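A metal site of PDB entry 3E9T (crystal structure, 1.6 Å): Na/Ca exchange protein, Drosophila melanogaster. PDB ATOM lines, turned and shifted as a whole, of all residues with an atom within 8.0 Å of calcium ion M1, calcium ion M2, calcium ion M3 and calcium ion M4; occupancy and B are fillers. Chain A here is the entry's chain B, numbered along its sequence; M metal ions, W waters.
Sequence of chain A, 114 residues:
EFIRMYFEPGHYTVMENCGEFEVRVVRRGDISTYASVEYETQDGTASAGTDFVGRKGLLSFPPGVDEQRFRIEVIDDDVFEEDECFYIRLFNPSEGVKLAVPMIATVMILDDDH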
ATOM      1  N   MET A  15     -25.650  35.227 -20.127  1.00  0.00           N
ATOM      2  CA  MET A  15     -25.819  34.291 -19.048  1.00  0.00           C
ATOM      3  C   MET A  15     -26.814  33.209 -19.459  1.00  0.00           C
ATOM      4  O   MET A  15     -27.787  33.501 -20.174  1.00  0.00           O
ATOM      5  CB  MET A  15     -26.352  35.021 -17.807  1.00  0.00           C
ATOM      6  CG  MET A  15     -25.450  36.115 -17.258  1.00  0.00           C
ATOM      7  SD  MET A  15     -23.724  35.643 -17.097  1.00  0.00           S
ATOM      8  CE  MET A  15     -23.752  34.490 -15.740  1.00  0.00           C
ATOM      9  N   GLU A  16     -26.606  31.995 -18.979  1.00  0.00           N
ATOM     10  CA  GLU A  16     -27.505  30.882 -19.295  1.00  0.00           C
ATOM     11  C   GLU A  16     -28.953  31.160 -18.902  1.00  0.00           C
ATOM     12  O   GLU A  16     -29.862  30.650 -19.538  1.00  0.00           O
ATOM     13  CB  GLU A  16     -27.030  29.598 -18.632  1.00  0.00           C
ATOM     14  CG  GLU A  16     -27.839  28.414 -19.119  1.00  0.00           C
ATOM     15  CD  GLU A  16     -27.460  27.127 -18.431  1.00  0.00           C
ATOM     16  OE1 GLU A  16     -27.191  26.140 -19.149  1.00  0.00           O
ATOM     17  OE2 GLU A  16     -27.440  27.101 -17.192  1.00  0.00           O
ATOM     18  N   ASN A  17     -29.161  31.966 -17.857  1.00  0.00           N
ATOM     19  CA  ASN A  17     -30.511  32.294 -17.395  1.00  0.00           C
ATOM     20  C   ASN A  17     -31.086  33.611 -17.941  1.00  0.00           C
ATOM     21  O   ASN A  17     -32.024  34.165 -17.361  1.00  0.00           O
ATOM     22  CB  ASN A  17     -30.570  32.274 -15.864  1.00  0.00           C
ATOM     23  CG  ASN A  17     -29.652  33.305 -15.224  1.00  0.00           C
ATOM     24  OD1 ASN A  17     -28.763  33.864 -15.887  1.00  0.00           O
ATOM     25  ND2 ASN A  17     -29.866  33.572 -13.950  1.00  0.00           N
ATOM     26  N   CYS A  18     -30.545  34.098 -19.069  1.00  0.00           N
ATOM     27  CA  CYS A  18     -30.981  35.370 -19.655  1.00  0.00           C
ATOM     28  C   CYS A  18     -32.372  35.288 -20.312  1.00  0.00           C
ATOM     29  O   CYS A  18     -33.013  36.321 -20.545  1.00  0.00           O
ATOM     30  CB  CYS A  18     -29.961  35.876 -20.684  1.00  0.00           C
ATOM     31  SG  CYS A  18     -29.921  34.985 -22.236  1.00  0.00           S
ATOM     32  N   THR A  45     -19.328  24.655 -29.243  1.00  0.00           N
ATOM     33  CA  THR A  45     -19.354  23.788 -28.057  1.00  0.00           C
ATOM     34  C   THR A  45     -20.724  23.827 -27.376  1.00  0.00           C
ATOM     35  O   THR A  45     -21.079  22.899 -26.642  1.00  0.00           O
ATOM     36  CB  THR A  45     -18.228  24.130 -27.057  1.00  0.00           C
ATOM     37  OG1 THR A  45     -18.179  25.545 -26.847  1.00  0.00           O
ATOM     38  CG2 THR A  45     -16.891  23.656 -27.608  1.00  0.00           C
ATOM     39  N   ALA A  46     -21.486  24.897 -27.618  1.00  0.00           N
ATOM     40  CA  ALA A  46     -22.899  24.956 -27.228  1.00  0.00           C
ATOM     41  C   ALA A  46     -23.773  24.446 -28.387  1.00  0.00           C
ATOM     42  O   ALA A  46     -23.463  24.689 -29.563  1.00  0.00           O
ATOM     43  CB  ALA A  46     -23.282  26.373 -26.856  1.00  0.00           C
ATOM     44  N   SER A  47     -24.858  23.754 -28.056  1.00  0.00           N
ATOM     45  CA  SER A  47     -25.630  23.022 -29.065  1.00  0.00           C
ATOM     46  C   SER A  47     -27.103  23.384 -29.088  1.00  0.00           C
ATOM     47  O   SER A  47     -27.716  23.518 -28.026  1.00  0.00           O
ATOM     48  CB  SER A  47     -25.500  21.524 -28.812  1.00  0.00           C
ATOM     49  OG  SER A  47     -24.141  21.140 -28.829  1.00  0.00           O
ATOM     50  N   THR A  50     -30.016  21.973 -26.611  1.00  0.00           N
ATOM     51  CA  THR A  50     -29.548  21.774 -25.245  1.00  0.00           C
ATOM     52  C   THR A  50     -29.167  23.110 -24.579  1.00  0.00           C
ATOM     53  O   THR A  50     -29.513  23.348 -23.429  1.00  0.00           O
ATOM     54  CB  THR A  50     -28.390  20.729 -25.130  1.00  0.00           C
ATOM     55  OG1 THR A  50     -27.209  21.242 -25.716  1.00  0.00           O
ATOM     56  CG2 THR A  50     -28.723  19.436 -25.847  1.00  0.00           C
ATOM     57  N   ASP A  51     -28.494  23.987 -25.325  1.00  0.00           N
ATOM     58  CA  ASP A  51     -27.989  25.261 -24.793  1.00  0.00           C
ATOM     59  C   ASP A  51     -28.709  26.493 -25.305  1.00  0.00           C
ATOM     60  O   ASP A  51     -28.737  27.539 -24.647  1.00  0.00           O
ATOM     61  CB  ASP A  51     -26.493  25.402 -25.090  1.00  0.00           C
ATOM     62  CG  ASP A  51     -25.696  24.279 -24.500  1.00  0.00           C
ATOM     63  OD1 ASP A  51     -25.137  23.482 -25.273  1.00  0.00           O
ATOM     64  OD2 ASP A  51     -25.686  24.182 -23.255  1.00  0.00           O
ATOM     65  N   PHE A  52     -29.281  26.383 -26.499  1.00  0.00           N
ATOM     66  CA  PHE A  52     -30.030  27.496 -27.071  1.00  0.00           C
ATOM     67  C   PHE A  52     -31.038  26.895 -28.022  1.00  0.00           C
ATOM     68  O   PHE A  52     -30.902  25.752 -28.403  1.00  0.00           O
ATOM     69  CB  PHE A  52     -29.117  28.479 -27.814  1.00  0.00           C
ATOM     70  CG  PHE A  52     -28.362  27.863 -29.004  1.00  0.00           C
ATOM     71  CD1 PHE A  52     -27.123  27.228 -28.818  1.00  0.00           C
ATOM     72  CD2 PHE A  52     -28.882  27.928 -30.283  1.00  0.00           C
ATOM     73  CE1 PHE A  52     -26.427  26.646 -29.895  1.00  0.00           C
ATOM     74  CE2 PHE A  52     -28.186  27.356 -31.370  1.00  0.00           C
ATOM     75  CZ  PHE A  52     -26.950  26.740 -31.163  1.00  0.00           C
ATOM     76  N   VAL A  74     -32.140  31.279 -25.057  1.00  0.00           N
ATOM     77  CA  VAL A  74     -31.078  30.521 -24.398  1.00  0.00           C
ATOM     78  C   VAL A  74     -31.749  29.555 -23.402  1.00  0.00           C
ATOM     79  O   VAL A  74     -32.721  29.924 -22.714  1.00  0.00           O
ATOM     80  CB  VAL A  74     -30.075  31.482 -23.706  1.00  0.00           C
ATOM     81  CG1 VAL A  74     -29.012  30.700 -22.926  1.00  0.00           C
ATOM     82  CG2 VAL A  74     -29.383  32.391 -24.762  1.00  0.00           C
ATOM     83  N   ILE A  75     -31.277  28.306 -23.408  1.00  0.00           N
ATOM     84  CA  ILE A  75     -31.879  27.248 -22.577  1.00  0.00           C
ATOM     85  C   ILE A  75     -31.200  27.174 -21.212  1.00  0.00           C
ATOM     86  O   ILE A  75     -29.998  26.981 -21.104  1.00  0.00           O
ATOM     87  CB  ILE A  75     -31.897  25.853 -23.288  1.00  0.00           C
ATOM     88  CG1 ILE A  75     -32.708  25.931 -24.593  1.00  0.00           C
ATOM     89  CG2 ILE A  75     -32.458  24.761 -22.330  1.00  0.00           C
ATOM     90  CD1 ILE A  75     -32.676  24.652 -25.433  1.00  0.00           C
ATOM     91  N   ASP A  76     -32.005  27.344 -20.160  1.00  0.00           N
ATOM     92  CA  ASP A  76     -31.496  27.296 -18.811  1.00  0.00           C
ATOM     93  C   ASP A  76     -31.637  25.881 -18.275  1.00  0.00           C
ATOM     94  O   ASP A  76     -32.638  25.223 -18.517  1.00  0.00           O
ATOM     95  CB  ASP A  76     -32.281  28.273 -17.914  1.00  0.00           C
ATOM     96  CG  ASP A  76     -31.581  28.572 -16.601  1.00  0.00           C
ATOM     97  OD1 ASP A  76     -32.223  29.183 -15.727  1.00  0.00           O
ATOM     98  OD2 ASP A  76     -30.394  28.217 -16.442  1.00  0.00           O
ATOM     99  N   ASP A  77     -30.630  25.410 -17.562  1.00  0.00           N
ATOM    100  CA  ASP A  77     -30.807  24.184 -16.770  1.00  0.00           C
ATOM    101  C   ASP A  77     -30.197  24.317 -15.377  1.00  0.00           C
ATOM    102  O   ASP A  77     -29.801  25.413 -14.961  1.00  0.00           O
ATOM    103  CB  ASP A  77     -30.334  22.923 -17.516  1.00  0.00           C
ATOM    104  CG  ASP A  77     -28.887  22.987 -17.946  1.00  0.00           C
ATOM    105  OD1 ASP A  77     -28.576  22.456 -19.033  1.00  0.00           O
ATOM    106  OD2 ASP A  77     -28.056  23.552 -17.209  1.00  0.00           O
ATOM    107  N   ASP A  78     -30.165  23.209 -14.637  1.00  0.00           N
ATOM    108  CA  ASP A  78     -29.638  23.212 -13.283  1.00  0.00           C
ATOM    109  C   ASP A  78     -28.273  22.535 -13.240  1.00  0.00           C
ATOM    110  O   ASP A  78     -27.706  22.309 -12.163  1.00  0.00           O
ATOM    111  CB  ASP A  78     -30.609  22.470 -12.337  1.00  0.00           C
ATOM    112  CG  ASP A  78     -31.896  23.257 -12.068  1.00  0.00           C
ATOM    113  OD1 ASP A  78     -32.110  24.336 -12.687  1.00  0.00           O
ATOM    114  OD2 ASP A  78     -32.704  22.794 -11.226  1.00  0.00           O
ATOM    115  N   VAL A  79     -27.747  22.213 -14.425  1.00  0.00           N
ATOM    116  CA  VAL A  79     -26.475  21.521 -14.561  1.00  0.00           C
ATOM    117  C   VAL A  79     -25.347  22.539 -14.759  1.00  0.00           C
ATOM    118  O   VAL A  79     -25.399  23.382 -15.655  1.00  0.00           O
ATOM    119  CB  VAL A  79     -26.499  20.545 -15.772  1.00  0.00           C
ATOM    120  CG1 VAL A  79     -25.201  19.762 -15.866  1.00  0.00           C
ATOM    121  CG2 VAL A  79     -27.694  19.579 -15.663  1.00  0.00           C
ATOM    122  N   PHE A  80     -24.320  22.444 -13.906  1.00  0.00           N
ATOM    123  CA  PHE A  80     -23.111  23.243 -14.080  1.00  0.00           C
ATOM    124  C   PHE A  80     -22.439  22.910 -15.414  1.00  0.00           C
ATOM    125  O   PHE A  80     -22.315  21.736 -15.778  1.00  0.00           O
ATOM    126  CB  PHE A  80     -22.130  22.984 -12.926  1.00  0.00           C
ATOM    127  CG  PHE A  80     -20.696  23.226 -13.290  1.00  0.00           C
ATOM    128  CD1 PHE A  80     -19.848  22.157 -13.572  1.00  0.00           C
ATOM    129  CD2 PHE A  80     -20.198  24.524 -13.397  1.00  0.00           C
ATOM    130  CE1 PHE A  80     -18.516  22.376 -13.933  1.00  0.00           C
ATOM    131  CE2 PHE A  80     -18.866  24.753 -13.758  1.00  0.00           C
ATOM    132  CZ  PHE A  80     -18.031  23.674 -14.022  1.00  0.00           C
ATOM    133  N   GLU A  81     -22.047  23.959 -16.137  1.00  0.00           N
ATOM    134  CA  GLU A  81     -21.262  23.816 -17.384  1.00  0.00           C
ATOM    135  C   GLU A  81     -20.143  24.860 -17.472  1.00  0.00           C
ATOM    136  O   GLU A  81     -20.249  25.936 -16.896  1.00  0.00           O
ATOM    137  CB  GLU A  81     -22.145  23.970 -18.627  1.00  0.00           C
ATOM    138  CG  GLU A  81     -23.307  22.992 -18.717  1.00  0.00           C
ATOM    139  CD  GLU A  81     -24.449  23.582 -19.487  1.00  0.00           C
ATOM    140  OE1 GLU A  81     -25.425  24.043 -18.847  1.00  0.00           O
ATOM    141  OE2 GLU A  81     -24.365  23.631 -20.739  1.00  0.00           O
ATOM    142  N   GLU A  82     -19.100  24.545 -18.227  1.00  0.00           N
ATOM    143  CA  GLU A  82     -18.047  25.495 -18.522  1.00  0.00           C
ATOM    144  C   GLU A  82     -18.548  26.531 -19.544  1.00  0.00           C
ATOM    145  O   GLU A  82     -19.638  26.354 -20.105  1.00  0.00           O
ATOM    146  CB  GLU A  82     -16.831  24.735 -19.044  1.00  0.00           C
ATOM    147  CG  GLU A  82     -16.437  23.589 -18.095  1.00  0.00           C
ATOM    148  CD  GLU A  82     -15.162  22.866 -18.485  1.00  0.00           C
ATOM    149  OE1 GLU A  82     -14.742  21.967 -17.724  1.00  0.00           O
ATOM    150  OE2 GLU A  82     -14.577  23.172 -19.553  1.00  0.00           O
ATOM    151  N   ASP A  83     -17.791  27.601 -19.781  1.00  0.00           N
ATOM    152  CA  ASP A  83     -18.188  28.571 -20.809  1.00  0.00           C
ATOM    153  C   ASP A  83     -18.246  27.849 -22.157  1.00  0.00           C
ATOM    154  O   ASP A  83     -17.334  27.105 -22.496  1.00  0.00           O
ATOM    155  CB  ASP A  83     -17.206  29.733 -20.944  1.00  0.00           C
ATOM    156  CG  ASP A  83     -17.107  30.568 -19.676  1.00  0.00           C
ATOM    157  OD1 ASP A  83     -17.878  30.312 -18.718  1.00  0.00           O
ATOM    158  OD2 ASP A  83     -16.233  31.480 -19.616  1.00  0.00           O
ATOM    159  N   GLU A  84     -19.311  28.080 -22.920  1.00  0.00           N
ATOM    160  CA  GLU A  84     -19.468  27.425 -24.231  1.00  0.00           C
ATOM    161  C   GLU A  84     -19.904  28.434 -25.274  1.00  0.00           C
ATOM    162  O   GLU A  84     -20.546  29.416 -24.942  1.00  0.00           O
ATOM    163  CB  GLU A  84     -20.469  26.285 -24.169  1.00  0.00           C
ATOM    164  CG  GLU A  84     -20.031  25.161 -23.242  1.00  0.00           C
ATOM    165  CD  GLU A  84     -20.997  23.993 -23.205  1.00  0.00           C
ATOM    166  OE1 GLU A  84     -22.208  24.190 -23.446  1.00  0.00           O
ATOM    167  OE2 GLU A  84     -20.526  22.873 -22.912  1.00  0.00           O
ATOM    168  N   ILE A 109     -21.917  31.613 -23.898  1.00  0.00           N
ATOM    169  CA  ILE A 109     -22.887  31.418 -22.847  1.00  0.00           C
ATOM    170  C   ILE A 109     -22.109  31.129 -21.566  1.00  0.00           C
ATOM    171  O   ILE A 109     -21.277  30.208 -21.519  1.00  0.00           O
ATOM    172  CB  ILE A 109     -23.851  30.222 -23.126  1.00  0.00           C
ATOM    173  CG1 ILE A 109     -24.646  30.400 -24.415  1.00  0.00           C
ATOM    174  CG2 ILE A 109     -24.827  30.030 -21.915  1.00  0.00           C
ATOM    175  CD1 ILE A 109     -25.356  29.107 -24.870  1.00  0.00           C
ATOM    176  N   LEU A 110     -22.384  31.924 -20.543  1.00  0.00           N
ATOM    177  CA  LEU A 110     -21.797  31.730 -19.218  1.00  0.00           C
ATOM    178  C   LEU A 110     -22.814  31.058 -18.317  1.00  0.00           C
ATOM    179  O   LEU A 110     -23.964  31.477 -18.275  1.00  0.00           O
ATOM    180  CB  LEU A 110     -21.388  33.068 -18.598  1.00  0.00           C
ATOM    181  CG  LEU A 110     -20.571  34.014 -19.489  1.00  0.00           C
ATOM    182  CD1 LEU A 110     -20.258  35.275 -18.716  1.00  0.00           C
ATOM    183  CD2 LEU A 110     -19.287  33.327 -20.008  1.00  0.00           C
ATOM    184  N   ASP A 111     -22.390  30.012 -17.623  1.00  0.00           N
ATOM    185  CA  ASP A 111     -23.275  29.226 -16.766  1.00  0.00           C
ATOM    186  C   ASP A 111     -23.555  29.970 -15.462  1.00  0.00           C
ATOM    187  O   ASP A 111     -22.733  30.775 -15.010  1.00  0.00           O
ATOM    188  CB  ASP A 111     -22.645  27.860 -16.487  1.00  0.00           C
ATOM    189  CG  ASP A 111     -23.654  26.797 -16.078  1.00  0.00           C
ATOM    190  OD1 ASP A 111     -24.360  26.252 -16.957  1.00  0.00           O
ATOM    191  OD2 ASP A 111     -23.712  26.471 -14.884  1.00  0.00           O
ATOM    192  N   ASP A 112     -24.704  29.687 -14.851  1.00  0.00           N
ATOM    193  CA  ASP A 112     -25.108  30.309 -13.582  1.00  0.00           C
ATOM    194  C   ASP A 112     -25.266  29.300 -12.434  1.00  0.00           C
ATOM    195  O   ASP A 112     -25.572  29.680 -11.301  1.00  0.00           O
ATOM    196  CB  ASP A 112     -26.420  31.093 -13.774  1.00  0.00           C
ATOM    197  CG  ASP A 112     -27.581  30.187 -14.185  1.00  0.00           C
ATOM    198  OD1 ASP A 112     -27.393  29.283 -15.034  1.00  0.00           O
ATOM    199  OD2 ASP A 112     -28.705  30.368 -13.661  1.00  0.00           O
ATOM    200  N   ASP A 113     -25.039  28.016 -12.734  1.00  0.00           N
ATOM    201  CA  ASP A 113     -25.313  26.913 -11.801  1.00  0.00           C
ATOM    202  C   ASP A 113     -24.128  26.569 -10.892  1.00  0.00           C
ATOM    203  O   ASP A 113     -23.122  25.991 -11.329  1.00  0.00           O
ATOM    204  CB  ASP A 113     -25.778  25.669 -12.579  1.00  0.00           C
ATOM    205  CG  ASP A 113     -26.914  25.986 -13.542  1.00  0.00           C
ATOM    206  OD1 ASP A 113     -27.903  26.623 -13.089  1.00  0.00           O
ATOM    207  OD2 ASP A 113     -26.842  25.612 -14.733  1.00  0.00           O
HETATM  208 CA    CA M   1     -26.344  25.039 -16.704  1.00  0.00          CA
HETATM  209 CA    CA M   2     -23.958  22.422 -22.884  1.00  0.00          CA
HETATM  210 CA    CA M   3     -28.914  27.442 -15.056  1.00  0.00          CA
HETATM  211 CA    CA M   4     -25.904  25.535 -21.043  1.00  0.00          CA
HETATM  212  O   HOH W   1     -23.216  20.629 -21.570  1.00  0.00           O
HETATM  213  O   HOH W   2     -23.113  21.668 -24.603  1.00  0.00           O
HETATM  214  O   HOH W   3     -27.684  24.025 -21.012  1.00  0.00           O
HETATM  215  O   HOH W   4     -27.488  27.378 -22.178  1.00  0.00           O
HETATM  216  O   HOH W   5     -24.349  27.183 -19.360  1.00  0.00           O
HETATM  217  O   HOH W   6     -23.855  26.463 -22.464  1.00  0.00           O
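The backbone carbonyl oxygen of Glu 84 is in hydrogen-bond range of the backbone NH of Ile 109 (2.8 Å). The backbone carbonyl oxygen (O) of Asp 51 lies within hydrogen-bond range of the backbone NH (N) of Ile 75, at 2.9 Å. OD2 of Asp 112 is in hydrogen-bond range of ND2 of Asn 17 (3.4 Å). N of Ser 47 lies close to OD1 of Asp 51 (2.8 Å). OG1 of Thr 50 sits close to OD1 of Asp 51 (3.1 Å). O of Leu 110 sits at hydrogen-bond distance from N of Glu 16 (2.8 Å).
Along chain A the residues within 4 Å of calcium ion M3 span positions 16 to 113.
Calcium ion M2 is bound by water W2 (2.1 Å), water W1 (2.3 Å), OD2 of Asp 51 (2.5 Å), OE2 of Glu 81 (2.5 Å), OE1 of Glu 84 (2.6 Å) and OD1 of Asp 51 (2.9 Å). Calcium ion M2 has six donor atoms within binding distance.
Water W2 lies within hydrogen-bond range of the backbone carbonyl oxygen of Thr 45 (3.1 Å) and the side-chain carboxylate of Glu 84 (3.3 Å). Water W4 bridges the backbone carbonyl oxygen of Ile 75 (2.8 Å) and the backbone carbonyl oxygen of Asp 51 (2.8 Å). Water W3 bridges the side-chain carboxylate of Asp 77 (2.7 Å) and the backbone carbonyl oxygen of Thr 50 (3.1 Å).
Calcium ion M1 is bound by OD2 of Asp 113 (2.1 Å), O of Val 79 (2.2 Å), OD2 of Asp 77 (2.3 Å), OD1 of Asp 111 (2.3 Å), OE2 of Glu 16 (2.4 Å), OE1 of Glu 81 (2.5 Å) and OE1 of Glu 16 (2.8 Å). Calcium ion M1 has seven donor atoms within binding distance.
Three residues have an atom within 4 Å of calcium ion M4: Glu 16, Asp 51 and Glu 81. The nearest printed residue that does not touch calcium ion M4 is Ile 75 (4.3 Å).
Calcium ion M3 is bound by OD2 of Asp 76 (2.2 Å). O of Asp 77 binds calcium ion M3 (2.2 Å). Calcium ion M3 is bound by OD1 of Asp 113 (2.4 Å). The side-chain carboxylate (OD1) of Asp 112 binds calcium ion M3. Calcium ion M3 is bound by the side-chain carboxylate (OE2) of Glu 16. Calcium ion M3 is bound by OD2 of Asp 113, at 2.8 Å. Calcium ion M3 has six donor atoms within binding distance.
Of the 26 residues printed, 3 come within 4 Å of calcium ion M2.
Calcium ion M4 is bound by water W3 (2.3 Å). The side-chain carboxylate (OE1) of Glu 16 binds calcium ion M4. Calcium ion M4 is bound by the side-chain carboxylate (OE2) of Glu 81, 2.5 Å away. The side-chain carboxylate (OD2) of Asp 51 is bound to calcium ion M4 (2.6 Å). Calcium ion M4 is bound by water W6 (2.7 Å). Calcium ion M4 is bound by water W4 (2.7 Å). The side-chain carboxylate (OE1) of Glu 81 is bound to calcium ion M4, at 2.7 Å. Calcium ion M4 is bound by water W5 (2.8 Å).
Six residues have an atom within 4 Å of calcium ion M1: Glu 16, Asp 77, Val 79, Glu 81, Asp 111 and Asp 113. The nearest printed residue that does not touch calcium ion M1 is Phe 80 (4.3 Å).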
